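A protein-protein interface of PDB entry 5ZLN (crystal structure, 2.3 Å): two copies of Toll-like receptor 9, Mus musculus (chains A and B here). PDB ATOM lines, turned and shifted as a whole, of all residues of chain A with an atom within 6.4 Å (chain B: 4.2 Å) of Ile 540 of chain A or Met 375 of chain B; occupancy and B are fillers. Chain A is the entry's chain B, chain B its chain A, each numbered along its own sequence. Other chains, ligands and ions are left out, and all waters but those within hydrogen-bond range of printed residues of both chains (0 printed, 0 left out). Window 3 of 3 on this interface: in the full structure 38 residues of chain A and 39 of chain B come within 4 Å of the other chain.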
ATOM      1  N   ASP A 510     -19.109 -11.998 -16.529  1.00  0.00           N
ATOM      2  CA  ASP A 510     -19.791 -11.703 -17.760  1.00  0.00           C
ATOM      3  C   ASP A 510     -18.923 -10.738 -18.563  1.00  0.00           C
ATOM      4  O   ASP A 510     -18.868  -9.555 -18.279  1.00  0.00           O
ATOM      5  CB  ASP A 510     -21.185 -11.110 -17.464  1.00  0.00           C
ATOM      6  CG  ASP A 510     -21.927 -10.719 -18.725  1.00  0.00           C
ATOM      7  OD1 ASP A 510     -22.965 -10.030 -18.632  1.00  0.00           O
ATOM      8  OD2 ASP A 510     -21.456 -11.092 -19.833  1.00  0.00           O
ATOM      9  N   PRO A 534     -21.471 -18.317 -18.280  1.00  0.00           N
ATOM     10  CA  PRO A 534     -22.112 -17.362 -19.181  1.00  0.00           C
ATOM     11  C   PRO A 534     -21.960 -17.730 -20.642  1.00  0.00           C
ATOM     12  O   PRO A 534     -22.892 -17.542 -21.416  1.00  0.00           O
ATOM     13  CB  PRO A 534     -21.370 -16.052 -18.892  1.00  0.00           C
ATOM     14  CG  PRO A 534     -20.835 -16.232 -17.518  1.00  0.00           C
ATOM     15  CD  PRO A 534     -20.441 -17.662 -17.451  1.00  0.00           C
ATOM     16  N   PHE A 535     -20.814 -18.293 -21.016  1.00  0.00           N
ATOM     17  CA  PHE A 535     -20.571 -18.627 -22.420  1.00  0.00           C
ATOM     18  C   PHE A 535     -21.429 -19.802 -22.890  1.00  0.00           C
ATOM     19  O   PHE A 535     -21.545 -20.020 -24.095  1.00  0.00           O
ATOM     20  CB  PHE A 535     -19.094 -18.956 -22.634  1.00  0.00           C
ATOM     21  CG  PHE A 535     -18.187 -17.763 -22.558  1.00  0.00           C
ATOM     22  CD1 PHE A 535     -18.148 -16.849 -23.598  1.00  0.00           C
ATOM     23  CD2 PHE A 535     -17.369 -17.566 -21.456  1.00  0.00           C
ATOM     24  CE1 PHE A 535     -17.319 -15.764 -23.537  1.00  0.00           C
ATOM     25  CE2 PHE A 535     -16.507 -16.482 -21.392  1.00  0.00           C
ATOM     26  CZ  PHE A 535     -16.490 -15.572 -22.432  1.00  0.00           C
ATOM     27  N   MET A 537     -24.672 -20.013 -22.137  1.00  0.00           N
ATOM     28  CA  MET A 537     -26.050 -19.514 -22.386  1.00  0.00           C
ATOM     29  C   MET A 537     -26.350 -19.392 -23.885  1.00  0.00           C
ATOM     30  O   MET A 537     -25.827 -18.506 -24.546  1.00  0.00           O
ATOM     31  CB  MET A 537     -26.261 -18.138 -21.770  1.00  0.00           C
ATOM     32  CG  MET A 537     -26.217 -18.140 -20.268  1.00  0.00           C
ATOM     33  SD  MET A 537     -26.808 -16.616 -19.556  1.00  0.00           S
ATOM     34  CE  MET A 537     -25.375 -15.584 -19.692  1.00  0.00           C
ATOM     35  N   LYS A 538     -27.224 -20.252 -24.400  1.00  0.00           N
ATOM     36  CA  LYS A 538     -27.525 -20.271 -25.826  1.00  0.00           C
ATOM     37  C   LYS A 538     -28.467 -19.115 -26.223  1.00  0.00           C
ATOM     38  O   LYS A 538     -29.685 -19.191 -26.053  1.00  0.00           O
ATOM     39  CB  LYS A 538     -28.095 -21.626 -26.254  1.00  0.00           C
ATOM     40  CG  LYS A 538     -27.034 -22.733 -26.226  1.00  0.00           C
ATOM     41  CD  LYS A 538     -27.596 -24.124 -26.562  1.00  0.00           C
ATOM     42  CE  LYS A 538     -27.126 -25.238 -25.606  1.00  0.00           C
ATOM     43  NZ  LYS A 538     -27.954 -25.275 -24.363  1.00  0.00           N
ATOM     44  N   GLY A 539     -27.881 -18.076 -26.792  1.00  0.00           N
ATOM     45  CA  GLY A 539     -28.630 -16.944 -27.266  1.00  0.00           C
ATOM     46  C   GLY A 539     -28.173 -15.628 -26.695  1.00  0.00           C
ATOM     47  O   GLY A 539     -28.580 -14.590 -27.155  1.00  0.00           O
ATOM     48  N   ILE A 540     -27.322 -15.667 -25.690  1.00  0.00           N
ATOM     49  CA  ILE A 540     -26.690 -14.461 -25.184  1.00  0.00           C
ATOM     50  C   ILE A 540     -25.191 -14.455 -25.491  1.00  0.00           C
ATOM     51  O   ILE A 540     -24.444 -15.372 -25.121  1.00  0.00           O
ATOM     52  CB  ILE A 540     -26.938 -14.334 -23.678  1.00  0.00           C
ATOM     53  CG1 ILE A 540     -28.439 -14.044 -23.497  1.00  0.00           C
ATOM     54  CG2 ILE A 540     -26.071 -13.214 -23.090  1.00  0.00           C
ATOM     55  CD1 ILE A 540     -28.862 -13.990 -22.058  1.00  0.00           C
ATOM     56  N   GLY A 541     -24.760 -13.407 -26.173  1.00  0.00           N
ATOM     57  CA  GLY A 541     -23.383 -13.325 -26.622  1.00  0.00           C
ATOM     58  C   GLY A 541     -22.504 -12.562 -25.671  1.00  0.00           C
ATOM     59  O   GLY A 541     -22.962 -12.059 -24.646  1.00  0.00           O
ATOM     60  N   HIS A 542     -21.231 -12.468 -26.022  1.00  0.00           N
ATOM     61  CA  HIS A 542     -20.209 -11.834 -25.157  1.00  0.00           C
ATOM     62  C   HIS A 542     -19.212 -11.094 -25.991  1.00  0.00           C
ATOM     63  O   HIS A 542     -19.293 -11.111 -27.233  1.00  0.00           O
ATOM     64  CB  HIS A 542     -19.545 -12.892 -24.283  1.00  0.00           C
ATOM     65  CG  HIS A 542     -20.518 -13.521 -23.360  1.00  0.00           C
ATOM     66  ND1 HIS A 542     -21.365 -14.529 -23.772  1.00  0.00           N
ATOM     67  CD2 HIS A 542     -20.901 -13.180 -22.114  1.00  0.00           C
ATOM     68  CE1 HIS A 542     -22.182 -14.828 -22.780  1.00  0.00           C
ATOM     69  NE2 HIS A 542     -21.913 -14.037 -21.756  1.00  0.00           N
ATOM     70  N   THR A 565     -19.476 -19.662 -29.434  1.00  0.00           N
ATOM     71  CA  THR A 565     -20.472 -19.013 -30.255  1.00  0.00           C
ATOM     72  C   THR A 565     -20.766 -17.627 -29.700  1.00  0.00           C
ATOM     73  O   THR A 565     -20.644 -17.388 -28.488  1.00  0.00           O
ATOM     74  CB  THR A 565     -21.764 -19.906 -30.369  1.00  0.00           C
ATOM     75  OG1 THR A 565     -22.590 -19.444 -31.441  1.00  0.00           O
ATOM     76  CG2 THR A 565     -22.574 -19.909 -29.121  1.00  0.00           C
ATOM     77  N   ARG A 566     -21.143 -16.725 -30.604  1.00  0.00           N
ATOM     78  CA  ARG A 566     -21.637 -15.423 -30.248  1.00  0.00           C
ATOM     79  C   ARG A 566     -20.652 -14.630 -29.393  1.00  0.00           C
ATOM     80  O   ARG A 566     -20.988 -14.081 -28.338  1.00  0.00           O
ATOM     81  CB  ARG A 566     -22.993 -15.558 -29.519  1.00  0.00           C
ATOM     82  CG  ARG A 566     -24.151 -15.992 -30.398  1.00  0.00           C
ATOM     83  CD  ARG A 566     -25.455 -15.629 -29.741  1.00  0.00           C
ATOM     84  NE  ARG A 566     -26.594 -15.770 -30.639  1.00  0.00           N
ATOM     85  CZ  ARG A 566     -27.273 -16.890 -30.843  1.00  0.00           C
ATOM     86  NH1 ARG A 566     -26.954 -18.029 -30.214  1.00  0.00           N
ATOM     87  NH2 ARG A 566     -28.292 -16.847 -31.686  1.00  0.00           N
ATOM     88  N   PHE B 318     -36.456 -13.968 -27.674  1.00  0.00           N
ATOM     89  CA  PHE B 318     -35.450 -13.018 -28.217  1.00  0.00           C
ATOM     90  C   PHE B 318     -35.993 -11.841 -29.010  1.00  0.00           C
ATOM     91  O   PHE B 318     -35.372 -11.386 -29.956  1.00  0.00           O
ATOM     92  CB  PHE B 318     -34.343 -13.765 -28.948  1.00  0.00           C
ATOM     93  CG  PHE B 318     -33.467 -14.519 -28.000  1.00  0.00           C
ATOM     94  CD1 PHE B 318     -32.495 -13.855 -27.291  1.00  0.00           C
ATOM     95  CD2 PHE B 318     -33.690 -15.873 -27.737  1.00  0.00           C
ATOM     96  CE1 PHE B 318     -31.712 -14.524 -26.386  1.00  0.00           C
ATOM     97  CE2 PHE B 318     -32.919 -16.550 -26.813  1.00  0.00           C
ATOM     98  CZ  PHE B 318     -31.931 -15.867 -26.134  1.00  0.00           C
ATOM     99  N   GLY B 348     -35.303 -14.637 -23.350  1.00  0.00           N
ATOM    100  CA  GLY B 348     -34.455 -13.639 -23.991  1.00  0.00           C
ATOM    101  C   GLY B 348     -35.117 -12.356 -24.472  1.00  0.00           C
ATOM    102  O   GLY B 348     -34.744 -11.793 -25.489  1.00  0.00           O
ATOM    103  N   PHE B 350     -35.447  -9.900 -22.050  1.00  0.00           N
ATOM    104  CA  PHE B 350     -34.606  -9.098 -21.153  1.00  0.00           C
ATOM    105  C   PHE B 350     -35.450  -8.109 -20.341  1.00  0.00           C
ATOM    106  O   PHE B 350     -35.632  -6.950 -20.735  1.00  0.00           O
ATOM    107  CB  PHE B 350     -33.450  -8.372 -21.867  1.00  0.00           C
ATOM    108  CG  PHE B 350     -32.585  -9.252 -22.737  1.00  0.00           C
ATOM    109  CD1 PHE B 350     -32.440 -10.632 -22.502  1.00  0.00           C
ATOM    110  CD2 PHE B 350     -31.847  -8.684 -23.790  1.00  0.00           C
ATOM    111  CE1 PHE B 350     -31.607 -11.408 -23.312  1.00  0.00           C
ATOM    112  CE2 PHE B 350     -31.013  -9.456 -24.607  1.00  0.00           C
ATOM    113  CZ  PHE B 350     -30.901 -10.809 -24.368  1.00  0.00           C
ATOM    114  N   LEU B 373     -38.898 -19.029 -19.545  1.00  0.00           N
ATOM    115  CA  LEU B 373     -38.554 -17.688 -19.122  1.00  0.00           C
ATOM    116  C   LEU B 373     -37.026 -17.533 -18.886  1.00  0.00           C
ATOM    117  O   LEU B 373     -36.588 -16.723 -18.042  1.00  0.00           O
ATOM    118  CB  LEU B 373     -39.322 -17.359 -17.852  1.00  0.00           C
ATOM    119  CG  LEU B 373     -40.844 -17.187 -18.101  1.00  0.00           C
ATOM    120  CD1 LEU B 373     -41.642 -17.389 -16.812  1.00  0.00           C
ATOM    121  CD2 LEU B 373     -41.091 -15.805 -18.689  1.00  0.00           C
ATOM    122  N   GLN B 374     -36.230 -18.275 -19.662  1.00  0.00           N
ATOM    123  CA  GLN B 374     -34.774 -18.295 -19.508  1.00  0.00           C
ATOM    124  C   GLN B 374     -34.162 -17.021 -20.053  1.00  0.00           C
ATOM    125  O   GLN B 374     -34.715 -16.393 -20.942  1.00  0.00           O
ATOM    126  CB  GLN B 374     -34.134 -19.451 -20.290  1.00  0.00           C
ATOM    127  CG  GLN B 374     -34.673 -20.827 -19.975  1.00  0.00           C
ATOM    128  CD  GLN B 374     -34.240 -21.899 -20.974  1.00  0.00           C
ATOM    129  OE1 GLN B 374     -33.064 -22.133 -21.165  1.00  0.00           O
ATOM    130  NE2 GLN B 374     -35.211 -22.560 -21.595  1.00  0.00           N
ATOM    131  N   MET B 375     -32.989 -16.679 -19.539  1.00  0.00           N
ATOM    132  CA  MET B 375     -32.116 -15.712 -20.191  1.00  0.00           C
ATOM    133  C   MET B 375     -32.816 -14.375 -20.295  1.00  0.00           C
ATOM    134  O   MET B 375     -32.786 -13.762 -21.339  1.00  0.00           O
ATOM    135  CB  MET B 375     -31.670 -16.232 -21.578  1.00  0.00           C
ATOM    136  CG  MET B 375     -30.730 -17.442 -21.483  1.00  0.00           C
ATOM    137  SD  MET B 375     -30.161 -18.033 -23.080  1.00  0.00           S
ATOM    138  CE  MET B 375     -31.622 -18.911 -23.651  1.00  0.00           C
ATOM    139  N   ASN B 376     -33.439 -13.932 -19.206  1.00  0.00           N
ATOM    140  CA  ASN B 376     -34.141 -12.655 -19.214  1.00  0.00           C
ATOM    141  C   ASN B 376     -33.541 -11.585 -18.302  1.00  0.00           C
ATOM    142  O   ASN B 376     -34.100 -10.503 -18.189  1.00  0.00           O
ATOM    143  CB  ASN B 376     -35.622 -12.883 -18.842  1.00  0.00           C
ATOM    144  CG  ASN B 376     -36.444 -13.268 -20.034  1.00  0.00           C
ATOM    145  OD1 ASN B 376     -36.448 -12.541 -21.041  1.00  0.00           O
ATOM    146  ND2 ASN B 376     -37.108 -14.433 -19.962  1.00  0.00           N
ATOM    147  N   PHE B 377     -32.405 -11.869 -17.673  1.00  0.00           N
ATOM    148  CA  PHE B 377     -31.816 -10.992 -16.656  1.00  0.00           C
ATOM    149  C   PHE B 377     -32.783 -10.635 -15.502  1.00  0.00           C
ATOM    150  O   PHE B 377     -32.709  -9.537 -14.895  1.00  0.00           O
ATOM    151  CB  PHE B 377     -31.237  -9.731 -17.297  1.00  0.00           C
ATOM    152  CG  PHE B 377     -30.138 -10.006 -18.273  1.00  0.00           C
ATOM    153  CD1 PHE B 377     -28.855 -10.257 -17.832  1.00  0.00           C
ATOM    154  CD2 PHE B 377     -30.383  -9.995 -19.629  1.00  0.00           C
ATOM    155  CE1 PHE B 377     -27.841 -10.518 -18.730  1.00  0.00           C
ATOM    156  CE2 PHE B 377     -29.368 -10.248 -20.536  1.00  0.00           C
ATOM    157  CZ  PHE B 377     -28.102 -10.516 -20.087  1.00  0.00           C
ATOM    158  N   SER B 398     -34.324 -20.910 -15.698  1.00  0.00           N
ATOM    159  CA  SER B 398     -32.867 -21.070 -15.630  1.00  0.00           C
ATOM    160  C   SER B 398     -32.164 -19.919 -16.339  1.00  0.00           C
ATOM    161  O   SER B 398     -32.756 -19.259 -17.186  1.00  0.00           O
ATOM    162  CB  SER B 398     -32.413 -22.411 -16.247  1.00  0.00           C
ATOM    163  OG  SER B 398     -32.821 -22.509 -17.586  1.00  0.00           O
ATOM    164  N   ASP B 399     -30.917 -19.656 -15.964  1.00  0.00           N
ATOM    165  CA  ASP B 399     -30.111 -18.564 -16.574  1.00  0.00           C
ATOM    166  C   ASP B 399     -30.764 -17.172 -16.360  1.00  0.00           C
ATOM    167  O   ASP B 399     -31.027 -16.415 -17.310  1.00  0.00           O
ATOM    168  CB  ASP B 399     -29.864 -18.816 -18.067  1.00  0.00           C
ATOM    169  CG  ASP B 399     -28.777 -19.870 -18.309  1.00  0.00           C
ATOM    170  OD1 ASP B 399     -27.615 -19.694 -17.831  1.00  0.00           O
ATOM    171  OD2 ASP B 399     -29.063 -20.882 -18.992  1.00  0.00           O
ATOM    172  N   ASN B 400     -31.043 -16.875 -15.098  1.00  0.00           N
ATOM    173  CA  ASN B 400     -31.491 -15.569 -14.693  1.00  0.00           C
ATOM    174  C   ASN B 400     -30.605 -15.100 -13.522  1.00  0.00           C
ATOM    175  O   ASN B 400     -29.558 -15.713 -13.259  1.00  0.00           O
ATOM    176  CB  ASN B 400     -32.978 -15.610 -14.387  1.00  0.00           C
ATOM    177  CG  ASN B 400     -33.812 -15.541 -15.652  1.00  0.00           C
ATOM    178  OD1 ASN B 400     -33.807 -14.517 -16.339  1.00  0.00           O
ATOM    179  ND2 ASN B 400     -34.508 -16.642 -15.994  1.00  0.00           N
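SD of Met 375 of chain B lies close to O of Lys 538 of chain A, 3.2 Å away. OD1 of Asp 399 of chain B sits close to SD of Met 537 of chain A (3.6 Å).
The backbone carbonyl oxygen (O) of Ile 540 of chain A sits close to a ring nitrogen (ND1) of His 542 of chain A (3.5 Å). The backbone NH (N) of Met 375 of chain B lies within hydrogen-bond range of the backbone carbonyl oxygen (O) of Asp 399 of chain B, at 3.0 Å. O of Ser 398 of chain B sits at hydrogen-bond distance from N of Met 375 of chain B. The backbone NH (N) of Gly 348 of chain B lies close to the backbone carbonyl oxygen (O) of Met 375 of chain B, 3.3 Å away. N of Phe 350 of chain B sits at hydrogen-bond distance from OD1 of Asn 376 of chain B (3.0 Å).
Among the printed residues, merely in contact across the chains: Gly 539 of chain A with Phe 318 of chain B (3.2 Å), Ile 540 of chain A with Met 375 of chain B (3.6 Å) and Ile 540 of chain A with Phe 350 of chain B (3.97 Å).
Of chain B, only Phe 350 and Met 375 come within 4 Å of Ile 540 of chain A. Printed residues of chain A within 4 Å of Phe 350 of chain B: Ile 540 (3.97 Å). Of the printed residues of chain B, Lys 538 of chain A touches Met 375 (3.1 Å). Of the printed residues of chain B, Met 537 of chain A touches Asp 399 (3.2 Å). Of the printed residues of chain A, Phe 318 of chain B touches Gly 539. Printed residues of chain B within 4 Å of Gly 539 of chain A: Phe 318 (3.2 Å). Thr 565 of chain A touches none of the printed residues of chain B. The nearest residue of chain A that does not touch Met 375 of chain B is Met 537 of chain A (4.1 Å). The nearest printed residue of chain B that does not touch Lys 538 of chain A is Phe 318 of chain B (4.01 Å).
Of the 11 printed residues of chain B, 4 touch a printed residue of chain A. Hydrophobic or aromatic side chains of chain B that line the printed part of chain A: Phe 318, Phe 350 and Met 375. Along chain A the printed residues that touch a printed residue of chain B span positions 537 to 540. Among the printed residues, 5 pairs touch across the chains. Among the printed residues, no Asp or Glu carboxylate lies within 4 Å of a Lys or Arg side-chain nitrogen of the other chain.
No position is printed for both chains. Of the 5 pairs that touch across the chains among the printed residues, none has its exchanged pair printed and touching as well.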
